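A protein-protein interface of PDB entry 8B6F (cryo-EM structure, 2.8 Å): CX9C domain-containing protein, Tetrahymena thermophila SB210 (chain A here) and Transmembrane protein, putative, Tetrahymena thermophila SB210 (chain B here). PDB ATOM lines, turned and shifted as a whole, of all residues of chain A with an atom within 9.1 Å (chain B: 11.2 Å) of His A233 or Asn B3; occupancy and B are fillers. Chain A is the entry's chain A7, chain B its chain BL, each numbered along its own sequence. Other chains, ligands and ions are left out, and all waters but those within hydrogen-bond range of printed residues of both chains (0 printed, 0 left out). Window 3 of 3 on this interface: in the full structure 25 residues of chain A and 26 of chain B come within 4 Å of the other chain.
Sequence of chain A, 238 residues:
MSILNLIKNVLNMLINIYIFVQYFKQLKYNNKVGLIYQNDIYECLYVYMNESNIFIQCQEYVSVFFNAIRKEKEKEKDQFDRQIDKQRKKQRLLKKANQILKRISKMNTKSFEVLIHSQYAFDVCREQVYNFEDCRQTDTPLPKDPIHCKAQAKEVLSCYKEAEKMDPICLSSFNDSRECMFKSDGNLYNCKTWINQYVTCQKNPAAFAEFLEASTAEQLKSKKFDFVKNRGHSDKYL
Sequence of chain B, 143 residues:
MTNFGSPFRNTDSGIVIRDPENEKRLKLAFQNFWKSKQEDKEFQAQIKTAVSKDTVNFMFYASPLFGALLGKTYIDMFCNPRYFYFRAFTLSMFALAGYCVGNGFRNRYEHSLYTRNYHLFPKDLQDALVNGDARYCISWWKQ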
ATOM      1  N   TYR A 189      -6.233  11.267  -1.883  1.00  0.00           N
ATOM      2  CA  TYR A 189      -7.402  10.440  -2.164  1.00  0.00           C
ATOM      3  C   TYR A 189      -7.645  10.318  -3.663  1.00  0.00           C
ATOM      4  O   TYR A 189      -7.954   9.230  -4.162  1.00  0.00           O
ATOM      5  CB  TYR A 189      -8.634  11.014  -1.466  1.00  0.00           C
ATOM      6  CG  TYR A 189      -9.831  10.099  -1.512  1.00  0.00           C
ATOM      7  CD1 TYR A 189     -10.728  10.143  -2.569  1.00  0.00           C
ATOM      8  CD2 TYR A 189     -10.065   9.189  -0.491  1.00  0.00           C
ATOM      9  CE1 TYR A 189     -11.821   9.304  -2.609  1.00  0.00           C
ATOM     10  CE2 TYR A 189     -11.154   8.348  -0.522  1.00  0.00           C
ATOM     11  CZ  TYR A 189     -12.028   8.408  -1.582  1.00  0.00           C
ATOM     12  OH  TYR A 189     -13.115   7.568  -1.610  1.00  0.00           O
ATOM     13  N   ASN A 190      -7.515  11.423  -4.399  1.00  0.00           N
ATOM     14  CA  ASN A 190      -7.780  11.385  -5.833  1.00  0.00           C
ATOM     15  C   ASN A 190      -6.803  10.475  -6.562  1.00  0.00           C
ATOM     16  O   ASN A 190      -7.153   9.894  -7.595  1.00  0.00           O
ATOM     17  CB  ASN A 190      -7.714  12.795  -6.420  1.00  0.00           C
ATOM     18  CG  ASN A 190      -8.821  13.693  -5.908  1.00  0.00           C
ATOM     19  OD1 ASN A 190      -9.870  13.219  -5.477  1.00  0.00           O
ATOM     20  ND2 ASN A 190      -8.594  15.000  -5.962  1.00  0.00           N
ATOM     21  N   PHE A 227      -7.585  18.023 -13.802  1.00  0.00           N
ATOM     22  CA  PHE A 227      -8.691  18.030 -12.850  1.00  0.00           C
ATOM     23  C   PHE A 227      -9.659  19.178 -13.110  1.00  0.00           C
ATOM     24  O   PHE A 227     -10.842  19.072 -12.770  1.00  0.00           O
ATOM     25  CB  PHE A 227      -8.146  18.082 -11.423  1.00  0.00           C
ATOM     26  CG  PHE A 227      -7.480  16.804 -10.993  1.00  0.00           C
ATOM     27  CD1 PHE A 227      -6.206  16.488 -11.435  1.00  0.00           C
ATOM     28  CD2 PHE A 227      -8.136  15.910 -10.164  1.00  0.00           C
ATOM     29  CE1 PHE A 227      -5.595  15.309 -11.049  1.00  0.00           C
ATOM     30  CE2 PHE A 227      -7.531  14.729  -9.775  1.00  0.00           C
ATOM     31  CZ  PHE A 227      -6.259  14.428 -10.218  1.00  0.00           C
ATOM     32  N   ASN A 230     -11.781  17.610 -15.622  1.00  0.00           N
ATOM     33  CA  ASN A 230     -12.453  16.479 -14.985  1.00  0.00           C
ATOM     34  C   ASN A 230     -12.342  16.647 -13.473  1.00  0.00           C
ATOM     35  O   ASN A 230     -11.444  16.096 -12.836  1.00  0.00           O
ATOM     36  CB  ASN A 230     -11.837  15.165 -15.448  1.00  0.00           C
ATOM     37  CG  ASN A 230     -11.642  15.112 -16.949  1.00  0.00           C
ATOM     38  OD1 ASN A 230     -12.455  15.632 -17.709  1.00  0.00           O
ATOM     39  ND2 ASN A 230     -10.558  14.481 -17.382  1.00  0.00           N
ATOM     40  N   ARG A 231     -13.271  17.417 -12.900  1.00  0.00           N
ATOM     41  CA  ARG A 231     -13.296  17.594 -11.451  1.00  0.00           C
ATOM     42  C   ARG A 231     -13.511  16.271 -10.726  1.00  0.00           C
ATOM     43  O   ARG A 231     -12.853  15.997  -9.715  1.00  0.00           O
ATOM     44  CB  ARG A 231     -14.385  18.594 -11.065  1.00  0.00           C
ATOM     45  CG  ARG A 231     -14.068  20.032 -11.441  1.00  0.00           C
ATOM     46  CD  ARG A 231     -15.205  20.668 -12.216  1.00  0.00           C
ATOM     47  NE  ARG A 231     -15.283  20.148 -13.575  1.00  0.00           N
ATOM     48  CZ  ARG A 231     -16.264  20.414 -14.425  1.00  0.00           C
ATOM     49  NH1 ARG A 231     -17.287  21.179 -14.084  1.00  0.00           N
ATOM     50  NH2 ARG A 231     -16.217  19.897 -15.650  1.00  0.00           N
ATOM     51  N   GLY A 232     -14.428  15.444 -11.219  1.00  0.00           N
ATOM     52  CA  GLY A 232     -14.769  14.202 -10.553  1.00  0.00           C
ATOM     53  C   GLY A 232     -16.188  14.213 -10.028  1.00  0.00           C
ATOM     54  O   GLY A 232     -17.072  14.825 -10.634  1.00  0.00           O
ATOM     55  N   HIS A 233     -16.422  13.545  -8.898  1.00  0.00           N
ATOM     56  CA  HIS A 233     -17.746  13.457  -8.289  1.00  0.00           C
ATOM     57  C   HIS A 233     -17.683  14.022  -6.877  1.00  0.00           C
ATOM     58  O   HIS A 233     -17.081  13.413  -5.987  1.00  0.00           O
ATOM     59  CB  HIS A 233     -18.251  12.015  -8.274  1.00  0.00           C
ATOM     60  CG  HIS A 233     -18.530  11.460  -9.635  1.00  0.00           C
ATOM     61  ND1 HIS A 233     -17.532  11.184 -10.546  1.00  0.00           N
ATOM     62  CD2 HIS A 233     -19.695  11.136 -10.244  1.00  0.00           C
ATOM     63  CE1 HIS A 233     -18.072  10.711 -11.654  1.00  0.00           C
ATOM     64  NE2 HIS A 233     -19.382  10.670 -11.497  1.00  0.00           N
ATOM     65  N   SER A 234     -18.314  15.176  -6.676  1.00  0.00           N
ATOM     66  CA  SER A 234     -18.472  15.766  -5.348  1.00  0.00           C
ATOM     67  C   SER A 234     -17.132  15.884  -4.626  1.00  0.00           C
ATOM     68  O   SER A 234     -17.000  15.555  -3.446  1.00  0.00           O
ATOM     69  CB  SER A 234     -19.469  14.952  -4.521  1.00  0.00           C
ATOM     70  OG  SER A 234     -19.608  15.488  -3.218  1.00  0.00           O
ATOM     71  N   ASP A 235     -16.126  16.368  -5.350  1.00  0.00           N
ATOM     72  CA  ASP A 235     -14.784  16.502  -4.793  1.00  0.00           C
ATOM     73  C   ASP A 235     -14.757  17.670  -3.818  1.00  0.00           C
ATOM     74  O   ASP A 235     -14.941  18.826  -4.214  1.00  0.00           O
ATOM     75  CB  ASP A 235     -13.766  16.701  -5.912  1.00  0.00           C
ATOM     76  CG  ASP A 235     -12.337  16.689  -5.409  1.00  0.00           C
ATOM     77  OD1 ASP A 235     -12.134  16.469  -4.197  1.00  0.00           O
ATOM     78  OD2 ASP A 235     -11.415  16.898  -6.224  1.00  0.00           O
ATOM     79  N   LYS A 236     -14.530  17.373  -2.539  1.00  0.00           N
ATOM     80  CA  LYS A 236     -14.408  18.404  -1.518  1.00  0.00           C
ATOM     81  C   LYS A 236     -13.008  19.001  -1.455  1.00  0.00           C
ATOM     82  O   LYS A 236     -12.821  20.032  -0.804  1.00  0.00           O
ATOM     83  CB  LYS A 236     -14.783  17.830  -0.150  1.00  0.00           C
ATOM     84  CG  LYS A 236     -14.721  18.837   0.991  1.00  0.00           C
ATOM     85  CD  LYS A 236     -15.130  18.202   2.305  1.00  0.00           C
ATOM     86  CE  LYS A 236     -14.949  19.170   3.456  1.00  0.00           C
ATOM     87  NZ  LYS A 236     -15.266  18.529   4.764  1.00  0.00           N
ATOM     88  N   TYR A 237     -12.032  18.395  -2.129  1.00  0.00           N
ATOM     89  CA  TYR A 237     -10.632  18.798  -2.006  1.00  0.00           C
ATOM     90  C   TYR A 237     -10.169  18.709  -0.554  1.00  0.00           C
ATOM     91  O   TYR A 237      -9.418  19.552  -0.062  1.00  0.00           O
ATOM     92  CB  TYR A 237     -10.417  20.203  -2.571  1.00  0.00           C
ATOM     93  CG  TYR A 237     -10.962  20.352  -3.969  1.00  0.00           C
ATOM     94  CD1 TYR A 237     -10.351  19.718  -5.043  1.00  0.00           C
ATOM     95  CD2 TYR A 237     -12.092  21.117  -4.217  1.00  0.00           C
ATOM     96  CE1 TYR A 237     -10.848  19.845  -6.326  1.00  0.00           C
ATOM     97  CE2 TYR A 237     -12.597  21.252  -5.496  1.00  0.00           C
ATOM     98  CZ  TYR A 237     -11.969  20.613  -6.547  1.00  0.00           C
ATOM     99  OH  TYR A 237     -12.465  20.741  -7.822  1.00  0.00           O
ATOM    100  N   THR B   2     -23.391   9.151 -12.887  1.00  0.00           N
ATOM    101  CA  THR B   2     -23.992   8.893 -11.550  1.00  0.00           C
ATOM    102  C   THR B   2     -23.773  10.088 -10.627  1.00  0.00           C
ATOM    103  O   THR B   2     -22.855  10.878 -10.829  1.00  0.00           O
ATOM    104  CB  THR B   2     -23.402   7.628 -10.905  1.00  0.00           C
ATOM    105  OG1 THR B   2     -21.976   7.740 -10.842  1.00  0.00           O
ATOM    106  CG2 THR B   2     -23.771   6.394 -11.709  1.00  0.00           C
ATOM    107  N   ASN B   3     -24.624  10.211  -9.608  1.00  0.00           N
ATOM    108  CA  ASN B   3     -24.537  11.355  -8.706  1.00  0.00           C
ATOM    109  C   ASN B   3     -23.226  11.353  -7.930  1.00  0.00           C
ATOM    110  O   ASN B   3     -22.510  12.359  -7.897  1.00  0.00           O
ATOM    111  CB  ASN B   3     -25.725  11.349  -7.743  1.00  0.00           C
ATOM    112  CG  ASN B   3     -27.056  11.461  -8.457  1.00  0.00           C
ATOM    113  OD1 ASN B   3     -27.128  11.348  -9.678  1.00  0.00           O
ATOM    114  ND2 ASN B   3     -28.119  11.676  -7.694  1.00  0.00           N
ATOM    115  N   PHE B   4     -22.893  10.223  -7.302  1.00  0.00           N
ATOM    116  CA  PHE B   4     -21.719  10.133  -6.447  1.00  0.00           C
ATOM    117  C   PHE B   4     -20.625   9.227  -6.987  1.00  0.00           C
ATOM    118  O   PHE B   4     -19.471   9.373  -6.575  1.00  0.00           O
ATOM    119  CB  PHE B   4     -22.118   9.631  -5.050  1.00  0.00           C
ATOM    120  CG  PHE B   4     -23.146  10.485  -4.370  1.00  0.00           C
ATOM    121  CD1 PHE B   4     -22.767  11.591  -3.627  1.00  0.00           C
ATOM    122  CD2 PHE B   4     -24.492  10.183  -4.473  1.00  0.00           C
ATOM    123  CE1 PHE B   4     -23.711  12.380  -3.000  1.00  0.00           C
ATOM    124  CE2 PHE B   4     -25.441  10.968  -3.847  1.00  0.00           C
ATOM    125  CZ  PHE B   4     -25.049  12.067  -3.111  1.00  0.00           C
ATOM    126  N   GLY B   5     -20.945   8.311  -7.890  1.00  0.00           N
ATOM    127  CA  GLY B   5     -19.950   7.370  -8.350  1.00  0.00           C
ATOM    128  C   GLY B   5     -19.680   6.308  -7.298  1.00  0.00           C
ATOM    129  O   GLY B   5     -20.426   6.125  -6.339  1.00  0.00           O
ATOM    130  N   SER B   6     -18.580   5.599  -7.502  1.00  0.00           N
ATOM    131  CA  SER B   6     -18.209   4.543  -6.577  1.00  0.00           C
ATOM    132  C   SER B   6     -17.830   5.147  -5.226  1.00  0.00           C
ATOM    133  O   SER B   6     -17.221   6.219  -5.174  1.00  0.00           O
ATOM    134  CB  SER B   6     -17.048   3.725  -7.134  1.00  0.00           C
ATOM    135  OG  SER B   6     -15.922   4.547  -7.375  1.00  0.00           O
ATOM    136  N   PRO B   7     -18.175   4.485  -4.117  1.00  0.00           N
ATOM    137  CA  PRO B   7     -17.797   5.022  -2.802  1.00  0.00           C
ATOM    138  C   PRO B   7     -16.342   4.793  -2.443  1.00  0.00           C
ATOM    139  O   PRO B   7     -15.822   5.500  -1.571  1.00  0.00           O
ATOM    140  CB  PRO B   7     -18.722   4.264  -1.842  1.00  0.00           C
ATOM    141  CG  PRO B   7     -18.937   2.959  -2.514  1.00  0.00           C
ATOM    142  CD  PRO B   7     -18.953   3.240  -3.996  1.00  0.00           C
ATOM    143  N   PHE B   8     -15.673   3.830  -3.076  1.00  0.00           N
ATOM    144  CA  PHE B   8     -14.301   3.508  -2.705  1.00  0.00           C
ATOM    145  C   PHE B   8     -13.312   4.532  -3.245  1.00  0.00           C
ATOM    146  O   PHE B   8     -12.322   4.849  -2.579  1.00  0.00           O
ATOM    147  CB  PHE B   8     -13.944   2.110  -3.209  1.00  0.00           C
ATOM    148  CG  PHE B   8     -14.977   1.072  -2.886  1.00  0.00           C
ATOM    149  CD1 PHE B   8     -15.044   0.511  -1.625  1.00  0.00           C
ATOM    150  CD2 PHE B   8     -15.881   0.656  -3.849  1.00  0.00           C
ATOM    151  CE1 PHE B   8     -15.994  -0.444  -1.326  1.00  0.00           C
ATOM    152  CE2 PHE B   8     -16.834  -0.298  -3.557  1.00  0.00           C
ATOM    153  CZ  PHE B   8     -16.890  -0.848  -2.293  1.00  0.00           C
ATOM    154  N   ARG B   9     -13.557   5.057  -4.443  1.00  0.00           N
ATOM    155  CA  ARG B   9     -12.630   5.964  -5.102  1.00  0.00           C
ATOM    156  C   ARG B   9     -13.406   7.129  -5.698  1.00  0.00           C
ATOM    157  O   ARG B   9     -14.630   7.091  -5.827  1.00  0.00           O
ATOM    158  CB  ARG B   9     -11.827   5.243  -6.190  1.00  0.00           C
ATOM    159  CG  ARG B   9     -12.688   4.698  -7.305  1.00  0.00           C
ATOM    160  CD  ARG B   9     -11.942   3.691  -8.152  1.00  0.00           C
ATOM    161  NE  ARG B   9     -12.808   3.123  -9.177  1.00  0.00           N
ATOM    162  CZ  ARG B   9     -13.708   2.175  -8.957  1.00  0.00           C
ATOM    163  NH1 ARG B   9     -13.893   1.662  -7.751  1.00  0.00           N
ATOM    164  NH2 ARG B   9     -14.445   1.732  -9.971  1.00  0.00           N
ATOM    165  N   ASN B  10     -12.672   8.179  -6.058  1.00  0.00           N
ATOM    166  CA  ASN B  10     -13.251   9.365  -6.686  1.00  0.00           C
ATOM    167  C   ASN B  10     -13.341   9.101  -8.183  1.00  0.00           C
ATOM    168  O   ASN B  10     -12.374   9.300  -8.922  1.00  0.00           O
ATOM    169  CB  ASN B  10     -12.405  10.595  -6.377  1.00  0.00           C
ATOM    170  CG  ASN B  10     -13.127  11.890  -6.677  1.00  0.00           C
ATOM    171  OD1 ASN B  10     -14.024  11.934  -7.516  1.00  0.00           O
ATOM    172  ND2 ASN B  10     -12.736  12.956  -5.992  1.00  0.00           N
ATOM    173  N   THR B  11     -14.508   8.650  -8.635  1.00  0.00           N
ATOM    174  CA  THR B  11     -14.674   8.247 -10.025  1.00  0.00           C
ATOM    175  C   THR B  11     -14.516   9.437 -10.964  1.00  0.00           C
ATOM    176  O   THR B  11     -15.005  10.536 -10.692  1.00  0.00           O
ATOM    177  CB  THR B  11     -16.045   7.599 -10.228  1.00  0.00           C
ATOM    178  OG1 THR B  11     -16.116   6.379  -9.480  1.00  0.00           O
ATOM    179  CG2 THR B  11     -16.297   7.292 -11.701  1.00  0.00           C
ATOM    180  N   ASP B  12     -13.833   9.201 -12.085  1.00  0.00           N
ATOM    181  CA  ASP B  12     -13.636  10.217 -13.120  1.00  0.00           C
ATOM    182  C   ASP B  12     -12.994  11.477 -12.548  1.00  0.00           C
ATOM    183  O   ASP B  12     -13.334  12.598 -12.933  1.00  0.00           O
ATOM    184  CB  ASP B  12     -14.954  10.552 -13.817  1.00  0.00           C
ATOM    185  CG  ASP B  12     -15.522   9.378 -14.587  1.00  0.00           C
ATOM    186  OD1 ASP B  12     -14.730   8.526 -15.042  1.00  0.00           O
ATOM    187  OD2 ASP B  12     -16.759   9.306 -14.741  1.00  0.00           O
ATOM    188  N   SER B  13     -12.053  11.295 -11.629  1.00  0.00           N
ATOM    189  CA  SER B  13     -11.314  12.398 -11.031  1.00  0.00           C
ATOM    190  C   SER B  13      -9.919  12.428 -11.640  1.00  0.00           C
ATOM    191  O   SER B  13      -9.185  11.437 -11.568  1.00  0.00           O
ATOM    192  CB  SER B  13     -11.239  12.244  -9.513  1.00  0.00           C
ATOM    193  OG  SER B  13     -10.625  13.372  -8.915  1.00  0.00           O
ATOM    194  N   GLY B  14      -9.556  13.560 -12.236  1.00  0.00           N
ATOM    195  CA  GLY B  14      -8.298  13.645 -12.944  1.00  0.00           C
ATOM    196  C   GLY B  14      -8.452  13.205 -14.383  1.00  0.00           C
ATOM    197  O   GLY B  14      -8.863  13.989 -15.243  1.00  0.00           O
ATOM    198  N   ILE B  15      -8.118  11.949 -14.656  1.00  0.00           N
ATOM    199  CA  ILE B  15      -8.276  11.351 -15.976  1.00  0.00           C
ATOM    200  C   ILE B  15      -9.587  10.580 -16.006  1.00  0.00           C
ATOM    201  O   ILE B  15      -9.941   9.894 -15.039  1.00  0.00           O
ATOM    202  CB  ILE B  15      -7.083  10.436 -16.315  1.00  0.00           C
ATOM    203  CG1 ILE B  15      -7.162   9.990 -17.778  1.00  0.00           C
ATOM    204  CG2 ILE B  15      -7.047   9.229 -15.380  1.00  0.00           C
ATOM    205  CD1 ILE B  15      -5.984   9.155 -18.239  1.00  0.00           C
ATOM    206  N   VAL B  16     -10.317  10.701 -17.110  1.00  0.00           N
ATOM    207  CA  VAL B  16     -11.569   9.976 -17.298  1.00  0.00           C
ATOM    208  C   VAL B  16     -11.274   8.688 -18.054  1.00  0.00           C
ATOM    209  O   VAL B  16     -10.660   8.712 -19.128  1.00  0.00           O
ATOM    210  CB  VAL B  16     -12.602  10.843 -18.040  1.00  0.00           C
ATOM    211  CG1 VAL B  16     -12.155  11.147 -19.469  1.00  0.00           C
ATOM    212  CG2 VAL B  16     -13.960  10.159 -18.041  1.00  0.00           C
ATOM    213  N   ILE B  17     -11.690   7.561 -17.485  1.00  0.00           N
ATOM    214  CA  ILE B  17     -11.386   6.241 -18.027  1.00  0.00           C
ATOM    215  C   ILE B  17     -12.692   5.548 -18.378  1.00  0.00           C
ATOM    216  O   ILE B  17     -13.595   5.447 -17.540  1.00  0.00           O
ATOM    217  CB  ILE B  17     -10.561   5.400 -17.034  1.00  0.00           C
ATOM    218  CG1 ILE B  17     -10.277   4.003 -17.597  1.00  0.00           C
ATOM    219  CG2 ILE B  17     -11.270   5.288 -15.691  1.00  0.00           C
ATOM    220  CD1 ILE B  17      -9.537   4.002 -18.916  1.00  0.00           C
ATOM    221  N   ARG B  18     -12.790   5.076 -19.618  1.00  0.00           N
ATOM    222  CA  ARG B  18     -13.940   4.319 -20.105  1.00  0.00           C
ATOM    223  C   ARG B  18     -13.410   2.986 -20.619  1.00  0.00           C
ATOM    224  O   ARG B  18     -12.903   2.905 -21.742  1.00  0.00           O
ATOM    225  CB  ARG B  18     -14.684   5.083 -21.195  1.00  0.00           C
ATOM    226  CG  ARG B  18     -15.316   6.384 -20.727  1.00  0.00           C
ATOM    227  CD  ARG B  18     -16.528   6.128 -19.847  1.00  0.00           C
ATOM    228  NE  ARG B  18     -17.239   7.361 -19.528  1.00  0.00           N
ATOM    229  CZ  ARG B  18     -16.981   8.135 -18.482  1.00  0.00           C
ATOM    230  NH1 ARG B  18     -16.024   7.836 -17.617  1.00  0.00           N
ATOM    231  NH2 ARG B  18     -17.700   9.238 -18.298  1.00  0.00           N
ATOM    232  N   GLU B  23     -14.700  -3.338 -17.027  1.00  0.00           N
ATOM    233  CA  GLU B  23     -15.918  -3.452 -16.232  1.00  0.00           C
ATOM    234  C   GLU B  23     -16.525  -4.842 -16.359  1.00  0.00           C
ATOM    235  O   GLU B  23     -16.937  -5.441 -15.361  1.00  0.00           O
ATOM    236  CB  GLU B  23     -16.926  -2.386 -16.660  1.00  0.00           C
ATOM    237  CG  GLU B  23     -16.444  -0.961 -16.446  1.00  0.00           C
ATOM    238  CD  GLU B  23     -17.449   0.068 -16.927  1.00  0.00           C
ATOM    239  OE1 GLU B  23     -18.549  -0.333 -17.361  1.00  0.00           O
ATOM    240  OE2 GLU B  23     -17.138   1.276 -16.874  1.00  0.00           O
ATOM    241  N   CYS B 100     -37.621   6.221  -9.817  1.00  0.00           N
ATOM    242  CA  CYS B 100     -36.430   6.754  -9.168  1.00  0.00           C
ATOM    243  C   CYS B 100     -36.306   6.237  -7.742  1.00  0.00           C
ATOM    244  O   CYS B 100     -35.219   5.838  -7.311  1.00  0.00           O
ATOM    245  CB  CYS B 100     -36.477   8.281  -9.181  1.00  0.00           C
ATOM    246  SG  CYS B 100     -35.120   9.085  -8.305  1.00  0.00           S
ATOM    247  N   VAL B 101     -37.406   6.244  -6.989  1.00  0.00           N
ATOM    248  CA  VAL B 101     -37.366   5.730  -5.623  1.00  0.00           C
ATOM    249  C   VAL B 101     -36.969   4.259  -5.630  1.00  0.00           C
ATOM    250  O   VAL B 101     -36.109   3.823  -4.856  1.00  0.00           O
ATOM    251  CB  VAL B 101     -38.721   5.950  -4.930  1.00  0.00           C
ATOM    252  CG1 VAL B 101     -38.736   5.310  -3.548  1.00  0.00           C
ATOM    253  CG2 VAL B 101     -39.031   7.433  -4.836  1.00  0.00           C
ATOM    254  N   ASN B 103     -35.386   2.470  -7.995  1.00  0.00           N
ATOM    255  CA  ASN B 103     -34.016   2.267  -8.452  1.00  0.00           C
ATOM    256  C   ASN B 103     -33.016   2.684  -7.383  1.00  0.00           C
ATOM    257  O   ASN B 103     -31.968   2.049  -7.223  1.00  0.00           O
ATOM    258  CB  ASN B 103     -33.776   3.040  -9.746  1.00  0.00           C
ATOM    259  CG  ASN B 103     -32.447   2.704 -10.384  1.00  0.00           C
ATOM    260  OD1 ASN B 103     -31.854   1.667 -10.095  1.00  0.00           O
ATOM    261  ND2 ASN B 103     -31.971   3.582 -11.258  1.00  0.00           N
ATOM    262  N   GLY B 104     -33.323   3.746  -6.638  1.00  0.00           N
ATOM    263  CA  GLY B 104     -32.481   4.113  -5.515  1.00  0.00           C
ATOM    264  C   GLY B 104     -32.442   3.043  -4.443  1.00  0.00           C
ATOM    265  O   GLY B 104     -31.387   2.759  -3.874  1.00  0.00           O
ATOM    266  N   ASN B 107     -30.149   0.327  -5.821  1.00  0.00           N
ATOM    267  CA  ASN B 107     -28.748   0.732  -5.844  1.00  0.00           C
ATOM    268  C   ASN B 107     -28.163   0.795  -4.441  1.00  0.00           C
ATOM    269  O   ASN B 107     -27.002   0.429  -4.230  1.00  0.00           O
ATOM    270  CB  ASN B 107     -28.603   2.082  -6.539  1.00  0.00           C
ATOM    271  CG  ASN B 107     -27.181   2.356  -6.973  1.00  0.00           C
ATOM    272  OD1 ASN B 107     -26.232   1.867  -6.365  1.00  0.00           O
ATOM    273  ND2 ASN B 107     -27.026   3.136  -8.032  1.00  0.00           N
ATOM    274  N   ARG B 108     -28.945   1.268  -3.470  1.00  0.00           N
ATOM    275  CA  ARG B 108     -28.477   1.266  -2.089  1.00  0.00           C
ATOM    276  C   ARG B 108     -28.322  -0.148  -1.552  1.00  0.00           C
ATOM    277  O   ARG B 108     -27.420  -0.406  -0.748  1.00  0.00           O
ATOM    278  CB  ARG B 108     -29.428   2.075  -1.210  1.00  0.00           C
ATOM    279  CG  ARG B 108     -29.368   3.563  -1.493  1.00  0.00           C
ATOM    280  CD  ARG B 108     -30.178   4.353  -0.492  1.00  0.00           C
ATOM    281  NE  ARG B 108     -31.617   4.207  -0.684  1.00  0.00           N
ATOM    282  CZ  ARG B 108     -32.373   3.292  -0.089  1.00  0.00           C
ATOM    283  NH1 ARG B 108     -31.860   2.400   0.743  1.00  0.00           N
ATOM    284  NH2 ARG B 108     -33.680   3.275  -0.334  1.00  0.00           N
ATOM    285  N   HIS B 111     -25.008  -1.197  -2.900  1.00  0.00           N
ATOM    286  CA  HIS B 111     -23.949  -0.539  -2.144  1.00  0.00           C
ATOM    287  C   HIS B 111     -23.732  -1.224  -0.805  1.00  0.00           C
ATOM    288  O   HIS B 111     -22.595  -1.490  -0.402  1.00  0.00           O
ATOM    289  CB  HIS B 111     -24.307   0.935  -1.942  1.00  0.00           C
ATOM    290  CG  HIS B 111     -23.379   1.666  -1.025  1.00  0.00           C
ATOM    291  ND1 HIS B 111     -23.493   1.611   0.348  1.00  0.00           N
ATOM    292  CD2 HIS B 111     -22.326   2.479  -1.280  1.00  0.00           C
ATOM    293  CE1 HIS B 111     -22.551   2.354   0.898  1.00  0.00           C
ATOM    294  NE2 HIS B 111     -21.829   2.893  -0.068  1.00  0.00           N
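O of Pro B7 lies within hydrogen-bond range of OH of Tyr A189 (3.4 Å).
The backbone carbonyl oxygen (O) of Phe B8 is in hydrogen-bond range of the side-chain hydroxyl (OH) of Tyr A189, at 3.0 Å.
ND2 of Asn B10 lies within hydrogen-bond range of OD1 of Asn A190 (2.9 Å).
The side-chain amide oxygen of Asn B10 lies within hydrogen-bond range of the backbone NH of His A233 (3.2 Å).
The backbone carbonyl oxygen (O) of Thr B11 sits at hydrogen-bond distance from a ring nitrogen (ND1) of His A233 (2.6 Å).
The backbone carbonyl oxygen (O) of Asp B12 lies close to the backbone NH (N) of Gly A232, 3.5 Å away.
O of Gly B14 lies within hydrogen-bond range of ND2 of Asn A230.
The side-chain hydroxyl (OG1) of Thr B2 lies within hydrogen-bond range of the backbone NH (N) of Gly B5 (3.2 Å).
OG of Ser B6 lies close to O of Arg B9, at 3.2 Å.
The side-chain hydroxyl (OG1) of Thr B11 sits at hydrogen-bond distance from the side-chain hydroxyl (OG) of Ser B6, 2.8 Å away.
The guanidinium group (NH1) of Arg B18 is in salt-bridge range of the side-chain carboxylate (OD1) of Asp B12 (3.0 Å).
The side-chain carboxylate (OD2) of Asp A235 lies within hydrogen-bond range of the side-chain amide nitrogen (ND2) of Asn A190 (3.4 Å).
OD1 of Asp A235 sits at hydrogen-bond distance from N of Tyr A237, 2.8 Å away.
Asn A190 touches Ser B13 (CG to OG, 3.5 Å).
Ser B13 touches Phe A227 (OG to CE2, 3.5 Å).
Phe A227 touches Gly B14 (CE2 to N, 3.4 Å).
Asp B12 touches Asn A230.
Asn A230 touches Val B16.
O of Arg A231 touches OG of Ser B13, 3.5 Å away.
Asn B10 touches Gly A232.
Thr B11 touches Gly A232.
Thr B2 touches His A233.
Gly B5 touches His A233 (N to CD2, 3.9 Å).
Printed residues of chain B within 4 Å of Phe A227: Ser B13 (3.5 Å) and Gly B14 (3.4 Å).
Printed residues of chain B within 4 Å of Asn A230: Asp B12, Gly B14 and Val B16.
Of chain B, only Thr B2, Asn B3, Phe B4, Gly B5, Asn B10, Thr B11 and Asp B12 come within 4 Å of His A233.
No residue of chain B comes within 4 Å of Ser A234.
Asp A235 touches one residue of chain B.
Thr B2 touches just one residue of chain A: His A233.
Of chain A, only His A233 comes within 4 Å of Asn B3.
Phe B4 touches one residue of chain A.
Ser B6 touches none of the printed residues of chain A.
Printed residues of chain A within 4 Å of Thr B11: Gly A232 (3.7 Å) and His A233 (2.6 Å).
Of the printed residues of chain A, Ser B13 touches Asn A190 (3.5 Å), Phe A227 (3.5 Å), Arg A231 (3.5 Å) and Gly A232 (3.9 Å).
Printed residues of chain A within 4 Å of Val B16: Asn A230.
The nearest residue of chain B that does not touch His A233 is Ser B13 (5.4 Å).
The nearest residue of chain A that does not touch Asn B3 is Ser A234 (5.2 Å).
Of the 11 printed residues of chain A, 8 touch a printed residue of chain B.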
